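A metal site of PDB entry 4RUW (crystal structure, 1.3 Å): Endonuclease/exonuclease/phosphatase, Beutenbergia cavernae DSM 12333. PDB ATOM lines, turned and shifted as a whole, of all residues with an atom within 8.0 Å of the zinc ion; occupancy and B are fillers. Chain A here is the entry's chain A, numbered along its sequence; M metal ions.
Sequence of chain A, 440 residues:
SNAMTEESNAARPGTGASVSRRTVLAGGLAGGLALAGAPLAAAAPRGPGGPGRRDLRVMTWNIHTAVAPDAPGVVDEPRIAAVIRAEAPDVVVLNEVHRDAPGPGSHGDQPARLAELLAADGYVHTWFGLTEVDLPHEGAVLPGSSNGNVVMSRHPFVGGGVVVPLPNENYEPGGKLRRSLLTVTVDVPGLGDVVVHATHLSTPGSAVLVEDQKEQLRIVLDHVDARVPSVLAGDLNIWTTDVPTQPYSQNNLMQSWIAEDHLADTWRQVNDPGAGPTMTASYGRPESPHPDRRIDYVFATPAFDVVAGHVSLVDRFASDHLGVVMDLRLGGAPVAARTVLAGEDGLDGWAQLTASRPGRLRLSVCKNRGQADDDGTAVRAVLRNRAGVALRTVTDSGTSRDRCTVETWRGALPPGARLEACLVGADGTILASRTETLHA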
ATOM      1  N   THR A  65     -23.325  -4.194 -36.415  1.00  0.00           N
ATOM      2  CA  THR A  65     -22.699  -4.938 -35.315  1.00  0.00           C
ATOM      3  C   THR A  65     -23.136  -6.403 -35.232  1.00  0.00           C
ATOM      4  O   THR A  65     -23.144  -6.986 -34.144  1.00  0.00           O
ATOM      5  CB  THR A  65     -22.836  -4.239 -33.944  1.00  0.00           C
ATOM      6  OG1 THR A  65     -24.221  -4.076 -33.581  1.00  0.00           O
ATOM      7  CG2 THR A  65     -22.173  -2.884 -33.977  1.00  0.00           C
ATOM      8  N   VAL A  75     -25.992 -11.080 -30.746  1.00  0.00           N
ATOM      9  CA  VAL A  75     -24.850 -10.740 -31.581  1.00  0.00           C
ATOM     10  C   VAL A  75     -24.445 -11.985 -32.368  1.00  0.00           C
ATOM     11  O   VAL A  75     -24.087 -13.005 -31.772  1.00  0.00           O
ATOM     12  CB  VAL A  75     -23.675 -10.236 -30.729  1.00  0.00           C
ATOM     13  CG1 VAL A  75     -22.533  -9.793 -31.619  1.00  0.00           C
ATOM     14  CG2 VAL A  75     -24.126  -9.081 -29.835  1.00  0.00           C
ATOM     15  N   GLU A  96     -19.767  -0.604 -39.257  1.00  0.00           N
ATOM     16  CA  GLU A  96     -20.435  -0.929 -37.994  1.00  0.00           C
ATOM     17  C   GLU A  96     -19.935  -2.238 -37.394  1.00  0.00           C
ATOM     18  O   GLU A  96     -20.713  -3.124 -37.037  1.00  0.00           O
ATOM     19  CB  GLU A  96     -21.951  -0.940 -38.164  1.00  0.00           C
ATOM     20  CG  GLU A  96     -22.535   0.440 -38.425  1.00  0.00           C
ATOM     21  CD  GLU A  96     -22.284   1.394 -37.280  1.00  0.00           C
ATOM     22  OE1 GLU A  96     -22.793   1.132 -36.162  1.00  0.00           O
ATOM     23  OE2 GLU A  96     -21.574   2.406 -37.478  1.00  0.00           O
ATOM     24  N   VAL A  97     -18.614  -2.343 -37.278  1.00  0.00           N
ATOM     25  CA  VAL A  97     -17.976  -3.452 -36.618  1.00  0.00           C
ATOM     26  C   VAL A  97     -17.403  -2.924 -35.302  1.00  0.00           C
ATOM     27  O   VAL A  97     -16.614  -1.983 -35.310  1.00  0.00           O
ATOM     28  CB  VAL A  97     -16.825  -4.044 -37.486  1.00  0.00           C
ATOM     29  CG1 VAL A  97     -16.252  -5.279 -36.825  1.00  0.00           C
ATOM     30  CG2 VAL A  97     -17.305  -4.349 -38.905  1.00  0.00           C
ATOM     31  N   HIS A  98     -17.836  -3.503 -34.182  1.00  0.00           N
ATOM     32  CA  HIS A  98     -17.379  -3.017 -32.882  1.00  0.00           C
ATOM     33  C   HIS A  98     -16.211  -3.828 -32.334  1.00  0.00           C
ATOM     34  O   HIS A  98     -16.061  -5.021 -32.617  1.00  0.00           O
ATOM     35  CB  HIS A  98     -18.499  -3.001 -31.842  1.00  0.00           C
ATOM     36  CG  HIS A  98     -19.403  -1.808 -31.960  1.00  0.00           C
ATOM     37  ND1 HIS A  98     -20.230  -1.407 -30.930  1.00  0.00           N
ATOM     38  CD2 HIS A  98     -19.588  -0.946 -32.980  1.00  0.00           C
ATOM     39  CE1 HIS A  98     -20.895  -0.315 -31.329  1.00  0.00           C
ATOM     40  NE2 HIS A  98     -20.523  -0.023 -32.561  1.00  0.00           N
ATOM     41  N   ARG A  99     -15.379  -3.157 -31.561  1.00  0.00           N
ATOM     42  CA  ARG A  99     -14.365  -3.828 -30.782  1.00  0.00           C
ATOM     43  C   ARG A  99     -14.498  -3.274 -29.375  1.00  0.00           C
ATOM     44  O   ARG A  99     -14.015  -2.188 -29.069  1.00  0.00           O
ATOM     45  CB  ARG A  99     -12.977  -3.582 -31.383  1.00  0.00           C
ATOM     46  CG  ARG A  99     -11.861  -4.308 -30.644  1.00  0.00           C
ATOM     47  CD  ARG A  99     -10.717  -4.655 -31.572  1.00  0.00           C
ATOM     48  NE  ARG A  99      -9.894  -3.500 -31.900  1.00  0.00           N
ATOM     49  CZ  ARG A  99      -8.890  -3.533 -32.775  1.00  0.00           C
ATOM     50  NH1 ARG A  99      -8.605  -4.664 -33.415  1.00  0.00           N
ATOM     51  NH2 ARG A  99      -8.178  -2.441 -33.030  1.00  0.00           N
ATOM     52  N   ASP A 100     -15.212  -4.020 -28.530  1.00  0.00           N
ATOM     53  CA  ASP A 100     -15.649  -3.546 -27.222  1.00  0.00           C
ATOM     54  C   ASP A 100     -15.031  -4.345 -26.078  1.00  0.00           C
ATOM     55  O   ASP A 100     -14.950  -5.566 -26.167  1.00  0.00           O
ATOM     56  CB  ASP A 100     -17.155  -3.693 -27.046  1.00  0.00           C
ATOM     57  CG  ASP A 100     -17.976  -2.899 -28.037  1.00  0.00           C
ATOM     58  OD1 ASP A 100     -17.495  -1.891 -28.614  1.00  0.00           O
ATOM     59  OD2 ASP A 100     -19.144  -3.304 -28.232  1.00  0.00           O
ATOM     60  N   ALA A 101     -14.668  -3.650 -25.002  1.00  0.00           N
ATOM     61  CA  ALA A 101     -14.343  -4.290 -23.731  1.00  0.00           C
ATOM     62  C   ALA A 101     -15.642  -4.848 -23.131  1.00  0.00           C
ATOM     63  O   ALA A 101     -16.731  -4.496 -23.559  1.00  0.00           O
ATOM     64  CB  ALA A 101     -13.709  -3.262 -22.804  1.00  0.00           C
ATOM     65  N   PRO A 104     -22.151  -3.937 -19.997  1.00  0.00           N
ATOM     66  CA  PRO A 104     -23.551  -4.069 -20.439  1.00  0.00           C
ATOM     67  C   PRO A 104     -23.727  -3.710 -21.903  1.00  0.00           C
ATOM     68  O   PRO A 104     -23.461  -2.586 -22.324  1.00  0.00           O
ATOM     69  CB  PRO A 104     -24.305  -3.083 -19.527  1.00  0.00           C
ATOM     70  CG  PRO A 104     -23.257  -2.207 -18.904  1.00  0.00           C
ATOM     71  CD  PRO A 104     -22.002  -3.020 -18.860  1.00  0.00           C
ATOM     72  N   GLY A 105     -24.147  -4.694 -22.689  1.00  0.00           N
ATOM     73  CA  GLY A 105     -24.399  -4.494 -24.104  1.00  0.00           C
ATOM     74  C   GLY A 105     -23.182  -4.625 -24.997  1.00  0.00           C
ATOM     75  O   GLY A 105     -23.283  -4.397 -26.198  1.00  0.00           O
ATOM     76  N   SER A 106     -22.044  -4.999 -24.428  1.00  0.00           N
ATOM     77  CA  SER A 106     -20.815  -5.135 -25.220  1.00  0.00           C
ATOM     78  C   SER A 106     -20.969  -6.113 -26.378  1.00  0.00           C
ATOM     79  O   SER A 106     -21.679  -7.107 -26.250  1.00  0.00           O
ATOM     80  CB  SER A 106     -19.657  -5.572 -24.325  1.00  0.00           C
ATOM     81  OG  SER A 106     -18.505  -5.865 -25.079  1.00  0.00           O
ATOM     82  N   HIS A 107     -20.307  -5.823 -27.490  1.00  0.00           N
ATOM     83  CA  HIS A 107     -20.297  -6.688 -28.670  1.00  0.00           C
ATOM     84  C   HIS A 107     -19.042  -7.541 -28.747  1.00  0.00           C
ATOM     85  O   HIS A 107     -18.866  -8.321 -29.686  1.00  0.00           O
ATOM     86  CB  HIS A 107     -20.394  -5.833 -29.937  1.00  0.00           C
ATOM     87  CG  HIS A 107     -21.700  -5.120 -30.082  1.00  0.00           C
ATOM     88  ND1 HIS A 107     -21.868  -3.802 -29.701  1.00  0.00           N
ATOM     89  CD2 HIS A 107     -22.899  -5.538 -30.552  1.00  0.00           C
ATOM     90  CE1 HIS A 107     -23.122  -3.441 -29.939  1.00  0.00           C
ATOM     91  NE2 HIS A 107     -23.769  -4.477 -30.441  1.00  0.00           N
ATOM     92  N   GLY A 108     -18.150  -7.385 -27.767  1.00  0.00           N
ATOM     93  CA  GLY A 108     -16.891  -8.098 -27.757  1.00  0.00           C
ATOM     94  C   GLY A 108     -15.969  -7.666 -28.896  1.00  0.00           C
ATOM     95  O   GLY A 108     -16.138  -6.589 -29.467  1.00  0.00           O
ATOM     96  N   GLN A 110     -15.359  -7.985 -32.279  1.00  0.00           N
ATOM     97  CA  GLN A 110     -15.944  -8.473 -33.523  1.00  0.00           C
ATOM     98  C   GLN A 110     -14.945  -8.713 -34.651  1.00  0.00           C
ATOM     99  O   GLN A 110     -15.091  -9.696 -35.387  1.00  0.00           O
ATOM    100  CB  GLN A 110     -17.122  -7.604 -33.976  1.00  0.00           C
ATOM    101  CG  GLN A 110     -18.162  -7.419 -32.891  1.00  0.00           C
ATOM    102  CD  GLN A 110     -19.471  -6.919 -33.445  1.00  0.00           C
ATOM    103  OE1 GLN A 110     -19.550  -5.806 -33.966  1.00  0.00           O
ATOM    104  NE2 GLN A 110     -20.512  -7.724 -33.333  1.00  0.00           N
ATOM    105  N   LEU A 135     -19.124   4.498 -27.096  1.00  0.00           N
ATOM    106  CA  LEU A 135     -20.443   4.692 -27.662  1.00  0.00           C
ATOM    107  C   LEU A 135     -21.523   4.238 -26.683  1.00  0.00           C
ATOM    108  O   LEU A 135     -21.310   3.316 -25.895  1.00  0.00           O
ATOM    109  CB  LEU A 135     -20.585   3.885 -28.957  1.00  0.00           C
ATOM    110  CG  LEU A 135     -19.595   4.195 -30.089  1.00  0.00           C
ATOM    111  CD1 LEU A 135     -18.308   3.384 -29.968  1.00  0.00           C
ATOM    112  CD2 LEU A 135     -20.228   3.973 -31.452  1.00  0.00           C
ATOM    113  N   PRO A 136     -22.694   4.872 -26.754  1.00  0.00           N
ATOM    114  CA  PRO A 136     -23.848   4.394 -25.992  1.00  0.00           C
ATOM    115  C   PRO A 136     -24.207   2.952 -26.396  1.00  0.00           C
ATOM    116  O   PRO A 136     -24.283   2.632 -27.576  1.00  0.00           O
ATOM    117  CB  PRO A 136     -24.959   5.362 -26.399  1.00  0.00           C
ATOM    118  CG  PRO A 136     -24.237   6.614 -26.783  1.00  0.00           C
ATOM    119  CD  PRO A 136     -22.981   6.125 -27.468  1.00  0.00           C
ATOM    120  N   HIS A 137     -24.389   2.108 -25.383  1.00  0.00           N
ATOM    121  CA  HIS A 137     -24.869   0.740 -25.553  1.00  0.00           C
ATOM    122  C   HIS A 137     -25.967   0.565 -24.510  1.00  0.00           C
ATOM    123  O   HIS A 137     -25.726   0.758 -23.323  1.00  0.00           O
ATOM    124  CB  HIS A 137     -23.753  -0.263 -25.247  1.00  0.00           C
ATOM    125  CG  HIS A 137     -22.737  -0.416 -26.342  1.00  0.00           C
ATOM    126  ND1 HIS A 137     -21.875   0.600 -26.713  1.00  0.00           N
ATOM    127  CD2 HIS A 137     -22.430  -1.476 -27.118  1.00  0.00           C
ATOM    128  CE1 HIS A 137     -21.087   0.164 -27.679  1.00  0.00           C
ATOM    129  NE2 HIS A 137     -21.404  -1.093 -27.954  1.00  0.00           N
ATOM    130  N   LEU A 142     -20.738   3.042 -22.963  1.00  0.00           N
ATOM    131  CA  LEU A 142     -20.020   1.844 -22.552  1.00  0.00           C
ATOM    132  C   LEU A 142     -18.529   2.125 -22.628  1.00  0.00           C
ATOM    133  O   LEU A 142     -17.969   2.258 -23.718  1.00  0.00           O
ATOM    134  CB  LEU A 142     -20.383   0.669 -23.455  1.00  0.00           C
ATOM    135  CG  LEU A 142     -19.656  -0.645 -23.190  1.00  0.00           C
ATOM    136  CD1 LEU A 142     -19.913  -1.129 -21.767  1.00  0.00           C
ATOM    137  CD2 LEU A 142     -20.045  -1.711 -24.214  1.00  0.00           C
ATOM    138  N   GLY A 144     -14.669   1.739 -22.967  1.00  0.00           N
ATOM    139  CA  GLY A 144     -13.853   0.760 -23.653  1.00  0.00           C
ATOM    140  C   GLY A 144     -14.488   0.207 -24.920  1.00  0.00           C
ATOM    141  O   GLY A 144     -13.964  -0.752 -25.493  1.00  0.00           O
ATOM    142  N   SER A 145     -15.595   0.802 -25.363  1.00  0.00           N
ATOM    143  CA  SER A 145     -16.207   0.368 -26.613  1.00  0.00           C
ATOM    144  C   SER A 145     -15.617   1.131 -27.793  1.00  0.00           C
ATOM    145  O   SER A 145     -15.043   2.208 -27.631  1.00  0.00           O
ATOM    146  CB  SER A 145     -17.726   0.560 -26.560  1.00  0.00           C
ATOM    147  OG  SER A 145     -18.080   1.912 -26.354  1.00  0.00           O
ATOM    148  N   SER A 146     -15.753   0.578 -28.982  1.00  0.00           N
ATOM    149  CA  SER A 146     -15.290   1.272 -30.180  1.00  0.00           C
ATOM    150  C   SER A 146     -15.985   0.738 -31.411  1.00  0.00           C
ATOM    151  O   SER A 146     -16.419  -0.405 -31.447  1.00  0.00           O
ATOM    152  CB  SER A 146     -13.782   1.128 -30.346  1.00  0.00           C
ATOM    153  OG  SER A 146     -13.407  -0.168 -30.753  1.00  0.00           O
ATOM    154  N   ASN A 147     -16.093   1.611 -32.404  1.00  0.00           N
ATOM    155  CA  ASN A 147     -16.582   1.234 -33.719  1.00  0.00           C
ATOM    156  C   ASN A 147     -15.468   1.412 -34.744  1.00  0.00           C
ATOM    157  O   ASN A 147     -14.636   2.312 -34.613  1.00  0.00           O
ATOM    158  CB  ASN A 147     -17.778   2.084 -34.130  1.00  0.00           C
ATOM    159  CG  ASN A 147     -18.339   1.672 -35.470  1.00  0.00           C
ATOM    160  OD1 ASN A 147     -18.971   0.643 -35.581  1.00  0.00           O
ATOM    161  ND2 ASN A 147     -18.047   2.445 -36.507  1.00  0.00           N
HETATM  162 ZN    ZN M   1     -20.495  -2.358 -29.206  1.00  0.00          ZN
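OD2 of Asp 100 binds the zinc ion (1.9 Å).
The zinc ion is bound by a ring nitrogen (ND1) of His 98, at 2.0 Å.
NE2 of His 137 binds the zinc ion.
ND1 of His 107 is bound to the zinc ion, 2.1 Å away.
The zinc ion has four donor atoms within binding distance.
Of the 22 residues printed, 4 come within 4 Å of the zinc ion.
Along chain A the residues within 4 Å of the zinc ion span positions 98 to 137.
The backbone NH of Ser 146 sits at hydrogen-bond distance from the side-chain carboxylate of Asp 100.
The backbone NH of Asp 100 sits at hydrogen-bond distance from the backbone carbonyl oxygen of Gly 108.
The side-chain amide oxygen of Gln 110 lies within hydrogen-bond range of the backbone NH of His 98 (2.9 Å).
The side-chain amide oxygen of Asn 147 lies close to a ring nitrogen (NE2) of His 98 (3.5 Å).
ND1 of His 137 is in hydrogen-bond range of O of Leu 135 (2.9 Å).
A ring nitrogen (NE2) of His 107 lies within hydrogen-bond range of the side-chain hydroxyl (OG1) of Thr 65 (3.2 Å).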
